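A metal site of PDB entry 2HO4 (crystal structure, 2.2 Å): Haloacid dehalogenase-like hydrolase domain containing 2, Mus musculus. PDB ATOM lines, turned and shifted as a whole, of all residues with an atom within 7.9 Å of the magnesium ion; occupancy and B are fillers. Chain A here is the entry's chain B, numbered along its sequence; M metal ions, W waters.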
ATOM      1  N   ASP A  13     -12.041  18.429  -5.381  1.00  0.00           N
ATOM      2  CA  ASP A  13     -13.181  19.295  -5.373  1.00  0.00           C
ATOM      3  C   ASP A  13     -12.794  20.760  -5.301  1.00  0.00           C
ATOM      4  O   ASP A  13     -11.979  21.167  -4.501  1.00  0.00           O
ATOM      5  CB  ASP A  13     -14.094  18.970  -4.210  1.00  0.00           C
ATOM      6  CG  ASP A  13     -15.504  19.452  -4.455  1.00  0.00           C
ATOM      7  OD1 ASP A  13     -15.941  19.323  -5.627  1.00  0.00           O
ATOM      8  OD2 ASP A  13     -16.169  19.960  -3.506  1.00  0.00           O
ATOM      9  N   LEU A  14     -13.440  21.557  -6.136  1.00  0.00           N
ATOM     10  CA  LEU A  14     -13.309  22.993  -6.107  1.00  0.00           C
ATOM     11  C   LEU A  14     -14.121  23.623  -4.992  1.00  0.00           C
ATOM     12  O   LEU A  14     -13.579  23.996  -3.967  1.00  0.00           O
ATOM     13  CB  LEU A  14     -13.749  23.526  -7.481  1.00  0.00           C
ATOM     14  CG  LEU A  14     -12.951  22.799  -8.554  1.00  0.00           C
ATOM     15  CD1 LEU A  14     -13.555  22.986  -9.880  1.00  0.00           C
ATOM     16  CD2 LEU A  14     -11.533  23.363  -8.539  1.00  0.00           C
ATOM     17  N   ASN A  15     -15.426  23.742  -5.174  1.00  0.00           N
ATOM     18  CA  ASN A  15     -16.257  24.510  -4.272  1.00  0.00           C
ATOM     19  C   ASN A  15     -16.176  23.951  -2.856  1.00  0.00           C
ATOM     20  O   ASN A  15     -16.588  22.819  -2.616  1.00  0.00           O
ATOM     21  CB  ASN A  15     -17.681  24.542  -4.806  1.00  0.00           C
ATOM     22  CG  ASN A  15     -17.875  25.571  -5.927  1.00  0.00           C
ATOM     23  OD1 ASN A  15     -17.684  26.784  -5.711  1.00  0.00           O
ATOM     24  ND2 ASN A  15     -18.243  25.099  -7.130  1.00  0.00           N
ATOM     25  N   GLY A  16     -15.620  24.716  -1.912  1.00  0.00           N
ATOM     26  CA  GLY A  16     -15.513  24.274  -0.509  1.00  0.00           C
ATOM     27  C   GLY A  16     -14.181  23.621  -0.142  1.00  0.00           C
ATOM     28  O   GLY A  16     -13.862  23.408   1.021  1.00  0.00           O
ATOM     29  N   THR A  17     -13.395  23.290  -1.146  1.00  0.00           N
ATOM     30  CA  THR A  17     -12.110  22.633  -0.910  1.00  0.00           C
ATOM     31  C   THR A  17     -10.966  23.587  -1.283  1.00  0.00           C
ATOM     32  O   THR A  17     -10.146  23.939  -0.417  1.00  0.00           O
ATOM     33  CB  THR A  17     -12.086  21.290  -1.644  1.00  0.00           C
ATOM     34  OG1 THR A  17     -13.007  20.440  -0.970  1.00  0.00           O
ATOM     35  CG2 THR A  17     -10.701  20.649  -1.615  1.00  0.00           C
ATOM     36  N   LEU A  18     -10.962  24.016  -2.540  1.00  0.00           N
ATOM     37  CA  LEU A  18     -10.008  24.998  -3.022  1.00  0.00           C
ATOM     38  C   LEU A  18     -10.364  26.417  -2.629  1.00  0.00           C
ATOM     39  O   LEU A  18      -9.444  27.232  -2.421  1.00  0.00           O
ATOM     40  CB  LEU A  18      -9.821  24.909  -4.533  1.00  0.00           C
ATOM     41  CG  LEU A  18      -8.986  23.712  -4.956  1.00  0.00           C
ATOM     42  CD1 LEU A  18      -8.548  23.818  -6.432  1.00  0.00           C
ATOM     43  CD2 LEU A  18      -7.790  23.639  -4.022  1.00  0.00           C
ATOM     44  N   HIS A  19     -11.665  26.715  -2.542  1.00  0.00           N
ATOM     45  CA  HIS A  19     -12.140  28.081  -2.373  1.00  0.00           C
ATOM     46  C   HIS A  19     -13.565  28.178  -1.851  1.00  0.00           C
ATOM     47  O   HIS A  19     -14.435  27.449  -2.322  1.00  0.00           O
ATOM     48  CB  HIS A  19     -12.026  28.839  -3.703  1.00  0.00           C
ATOM     49  CG  HIS A  19     -12.943  28.325  -4.785  1.00  0.00           C
ATOM     50  ND1 HIS A  19     -14.255  28.724  -4.900  1.00  0.00           N
ATOM     51  CD2 HIS A  19     -12.727  27.458  -5.801  1.00  0.00           C
ATOM     52  CE1 HIS A  19     -14.808  28.125  -5.935  1.00  0.00           C
ATOM     53  NE2 HIS A  19     -13.906  27.345  -6.501  1.00  0.00           N
ATOM     54  N   VAL A  45     -12.669  18.538  -9.886  1.00  0.00           N
ATOM     55  CA  VAL A  45     -14.035  18.003 -10.066  1.00  0.00           C
ATOM     56  C   VAL A  45     -15.075  18.893  -9.383  1.00  0.00           C
ATOM     57  O   VAL A  45     -14.812  19.491  -8.341  1.00  0.00           O
ATOM     58  CB  VAL A  45     -14.205  16.471  -9.609  1.00  0.00           C
ATOM     59  CG1 VAL A  45     -13.403  15.537 -10.475  1.00  0.00           C
ATOM     60  CG2 VAL A  45     -13.885  16.253  -8.154  1.00  0.00           C
ATOM     61  N   THR A  46     -16.273  18.959  -9.993  1.00  0.00           N
ATOM     62  CA  THR A  46     -17.374  19.822  -9.562  1.00  0.00           C
ATOM     63  C   THR A  46     -18.661  19.291 -10.209  1.00  0.00           C
ATOM     64  O   THR A  46     -18.648  18.792 -11.356  1.00  0.00           O
ATOM     65  CB  THR A  46     -17.127  21.363  -9.884  1.00  0.00           C
ATOM     66  OG1 THR A  46     -18.290  22.126  -9.543  1.00  0.00           O
ATOM     67  CG2 THR A  46     -16.832  21.632 -11.318  1.00  0.00           C
ATOM     68  N   ASN A  47     -19.771  19.394  -9.461  1.00  0.00           N
ATOM     69  CA  ASN A  47     -21.109  18.893  -9.884  1.00  0.00           C
ATOM     70  C   ASN A  47     -22.005  20.004 -10.469  1.00  0.00           C
ATOM     71  O   ASN A  47     -23.230  20.032 -10.231  1.00  0.00           O
ATOM     72  CB  ASN A  47     -21.806  18.266  -8.666  1.00  0.00           C
ATOM     73  CG  ASN A  47     -22.407  16.934  -8.950  1.00  0.00           C
ATOM     74  OD1 ASN A  47     -22.045  16.274  -9.931  1.00  0.00           O
ATOM     75  ND2 ASN A  47     -23.316  16.490  -8.070  1.00  0.00           N
ATOM     76  N   LYS A 179     -21.853  13.554  -9.328  1.00  0.00           N
ATOM     77  CA  LYS A 179     -21.598  13.068  -7.964  1.00  0.00           C
ATOM     78  C   LYS A 179     -22.924  12.989  -7.227  1.00  0.00           C
ATOM     79  O   LYS A 179     -23.773  13.870  -7.376  1.00  0.00           O
ATOM     80  CB  LYS A 179     -20.724  14.044  -7.167  1.00  0.00           C
ATOM     81  CG  LYS A 179     -19.467  14.380  -7.799  1.00  0.00           C
ATOM     82  CD  LYS A 179     -19.068  15.813  -7.468  1.00  0.00           C
ATOM     83  CE  LYS A 179     -18.327  15.944  -6.155  1.00  0.00           C
ATOM     84  NZ  LYS A 179     -17.981  17.384  -6.031  1.00  0.00           N
ATOM     85  N   MET A 201      -9.157  11.164  -3.718  1.00  0.00           N
ATOM     86  CA  MET A 201     -10.088  12.238  -3.988  1.00  0.00           C
ATOM     87  C   MET A 201     -10.082  13.120  -2.764  1.00  0.00           C
ATOM     88  O   MET A 201     -10.073  12.567  -1.661  1.00  0.00           O
ATOM     89  CB  MET A 201     -11.506  11.643  -4.234  1.00  0.00           C
ATOM     90  CG  MET A 201     -12.668  12.577  -3.965  1.00  0.00           C
ATOM     91  SD  MET A 201     -12.887  13.825  -5.424  1.00  0.00           S
ATOM     92  CE  MET A 201     -13.958  14.951  -4.355  1.00  0.00           C
ATOM     93  N   ILE A 202     -10.053  14.460  -2.936  1.00  0.00           N
ATOM     94  CA  ILE A 202     -10.178  15.406  -1.769  1.00  0.00           C
ATOM     95  C   ILE A 202     -11.468  16.262  -1.886  1.00  0.00           C
ATOM     96  O   ILE A 202     -11.690  16.932  -2.873  1.00  0.00           O
ATOM     97  CB  ILE A 202      -8.889  16.372  -1.580  1.00  0.00           C
ATOM     98  CG1 ILE A 202      -7.582  15.581  -1.465  1.00  0.00           C
ATOM     99  CG2 ILE A 202      -8.956  17.127  -0.264  1.00  0.00           C
ATOM    100  CD1 ILE A 202      -6.464  16.045  -2.421  1.00  0.00           C
ATOM    101  N   GLY A 203     -12.336  16.220  -0.878  1.00  0.00           N
ATOM    102  CA  GLY A 203     -13.507  17.059  -0.911  1.00  0.00           C
ATOM    103  C   GLY A 203     -14.043  17.399   0.453  1.00  0.00           C
ATOM    104  O   GLY A 203     -13.638  16.822   1.456  1.00  0.00           O
ATOM    105  N   ASP A 204     -14.968  18.353   0.473  1.00  0.00           N
ATOM    106  CA  ASP A 204     -15.546  18.836   1.733  1.00  0.00           C
ATOM    107  C   ASP A 204     -16.848  18.121   2.127  1.00  0.00           C
ATOM    108  O   ASP A 204     -17.271  18.184   3.284  1.00  0.00           O
ATOM    109  CB  ASP A 204     -15.697  20.355   1.728  1.00  0.00           C
ATOM    110  CG  ASP A 204     -16.738  20.871   0.722  1.00  0.00           C
ATOM    111  OD1 ASP A 204     -16.727  20.505  -0.478  1.00  0.00           O
ATOM    112  OD2 ASP A 204     -17.531  21.727   1.182  1.00  0.00           O
ATOM    113  N   ASP A 205     -17.446  17.416   1.162  1.00  0.00           N
ATOM    114  CA  ASP A 205     -18.681  16.628   1.356  1.00  0.00           C
ATOM    115  C   ASP A 205     -18.400  15.126   1.564  1.00  0.00           C
ATOM    116  O   ASP A 205     -17.989  14.406   0.637  1.00  0.00           O
ATOM    117  CB  ASP A 205     -19.608  16.855   0.177  1.00  0.00           C
ATOM    118  CG  ASP A 205     -21.075  16.622   0.523  1.00  0.00           C
ATOM    119  OD1 ASP A 205     -21.418  15.499   0.979  1.00  0.00           O
ATOM    120  OD2 ASP A 205     -21.872  17.571   0.315  1.00  0.00           O
ATOM    121  N   ASP A 208     -20.905  13.057  -1.120  1.00  0.00           N
ATOM    122  CA  ASP A 208     -20.700  13.266  -2.553  1.00  0.00           C
ATOM    123  C   ASP A 208     -19.256  13.069  -2.955  1.00  0.00           C
ATOM    124  O   ASP A 208     -18.942  12.652  -4.096  1.00  0.00           O
ATOM    125  CB  ASP A 208     -21.162  14.663  -2.983  1.00  0.00           C
ATOM    126  CG  ASP A 208     -22.669  14.833  -2.908  1.00  0.00           C
ATOM    127  OD1 ASP A 208     -23.278  14.256  -1.959  1.00  0.00           O
ATOM    128  OD2 ASP A 208     -23.252  15.540  -3.773  1.00  0.00           O
ATOM    129  N   ASP A 209     -18.368  13.360  -2.012  1.00  0.00           N
ATOM    130  CA  ASP A 209     -16.953  13.386  -2.305  1.00  0.00           C
ATOM    131  C   ASP A 209     -16.263  12.083  -1.893  1.00  0.00           C
ATOM    132  O   ASP A 209     -15.794  11.342  -2.744  1.00  0.00           O
ATOM    133  CB  ASP A 209     -16.295  14.611  -1.644  1.00  0.00           C
ATOM    134  CG  ASP A 209     -16.695  15.927  -2.294  1.00  0.00           C
ATOM    135  OD1 ASP A 209     -16.953  15.944  -3.525  1.00  0.00           O
ATOM    136  OD2 ASP A 209     -16.700  16.962  -1.587  1.00  0.00           O
ATOM    137  N   THR A 225     -13.023  22.164   5.625  1.00  0.00           N
ATOM    138  CA  THR A 225     -13.452  23.486   5.135  1.00  0.00           C
ATOM    139  C   THR A 225     -14.774  23.344   4.389  1.00  0.00           C
ATOM    140  O   THR A 225     -15.309  22.245   4.258  1.00  0.00           O
ATOM    141  CB  THR A 225     -12.415  24.053   4.152  1.00  0.00           C
ATOM    142  OG1 THR A 225     -12.194  23.083   3.099  1.00  0.00           O
ATOM    143  CG2 THR A 225     -11.097  24.366   4.867  1.00  0.00           C
ATOM    144  N   GLY A 226     -15.278  24.458   3.885  1.00  0.00           N
ATOM    145  CA  GLY A 226     -16.468  24.417   3.032  1.00  0.00           C
ATOM    146  C   GLY A 226     -17.673  23.919   3.805  1.00  0.00           C
ATOM    147  O   GLY A 226     -17.884  24.356   4.905  1.00  0.00           O
ATOM    148  N   LYS A 227     -18.410  22.959   3.244  1.00  0.00           N
ATOM    149  CA  LYS A 227     -19.666  22.489   3.847  1.00  0.00           C
ATOM    150  C   LYS A 227     -19.497  21.682   5.140  1.00  0.00           C
ATOM    151  O   LYS A 227     -20.436  21.555   5.928  1.00  0.00           O
ATOM    152  CB  LYS A 227     -20.483  21.685   2.830  1.00  0.00           C
ATOM    153  CG  LYS A 227     -21.419  22.582   1.988  1.00  0.00           C
ATOM    154  CD  LYS A 227     -22.304  21.772   1.035  1.00  0.00           C
ATOM    155  CE  LYS A 227     -21.651  21.565  -0.353  1.00  0.00           C
ATOM    156  NZ  LYS A 227     -22.637  21.177  -1.424  1.00  0.00           N
ATOM    157  N   TYR A 228     -18.283  21.173   5.349  1.00  0.00           N
ATOM    158  CA  TYR A 228     -17.993  20.240   6.442  1.00  0.00           C
ATOM    159  C   TYR A 228     -18.477  20.722   7.789  1.00  0.00           C
ATOM    160  O   TYR A 228     -18.351  21.908   8.106  1.00  0.00           O
ATOM    161  CB  TYR A 228     -16.486  19.910   6.519  1.00  0.00           C
ATOM    162  CG  TYR A 228     -16.138  19.222   7.811  1.00  0.00           C
ATOM    163  CD1 TYR A 228     -15.980  19.952   8.992  1.00  0.00           C
ATOM    164  CD2 TYR A 228     -16.015  17.851   7.879  1.00  0.00           C
ATOM    165  CE1 TYR A 228     -15.707  19.320  10.196  1.00  0.00           C
ATOM    166  CE2 TYR A 228     -15.710  17.221   9.068  1.00  0.00           C
ATOM    167  CZ  TYR A 228     -15.561  17.962  10.214  1.00  0.00           C
ATOM    168  OH  TYR A 228     -15.265  17.334  11.379  1.00  0.00           O
HETATM  169 MG    MG M   1     -17.736  20.805  -2.416  1.00  0.00          MG
HETATM  170  O   HOH W   1     -19.003  21.849  -1.472  1.00  0.00           O
HETATM  171  O   HOH W   2     -18.150  18.687  -2.428  1.00  0.00           O
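The side-chain amino group of Lys 179 lies within salt-bridge range of the side-chain carboxylate of Asp 13. N of Asp 13 sits at hydrogen-bond distance from O of Ile 202 (2.9 Å). The side-chain carboxylate of Asp 209 lies within hydrogen-bond range of the backbone NH of Asp 204, at 3.0 Å. The side-chain carboxylate (OD2) of Asp 204 lies within hydrogen-bond range of the backbone NH (N) of Lys 227 (2.6 Å). OG1 of Thr 17 sits at hydrogen-bond distance from N of Asp 204, 3.2 Å away.
Along chain A the residues within 4 Å of the magnesium ion span positions 13 to 204. The nearest printed residue that does not touch the magnesium ion is Asp 209 (4.1 Å).
The magnesium ion is bound by water W1 (1.9 Å), OD2 of Asp 13 (2.1 Å), water W2 (2.2 Å), OD1 of Asp 204 (2.2 Å) and O of Asn 15 (2.3 Å). The magnesium ion has five donor atoms within binding distance.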
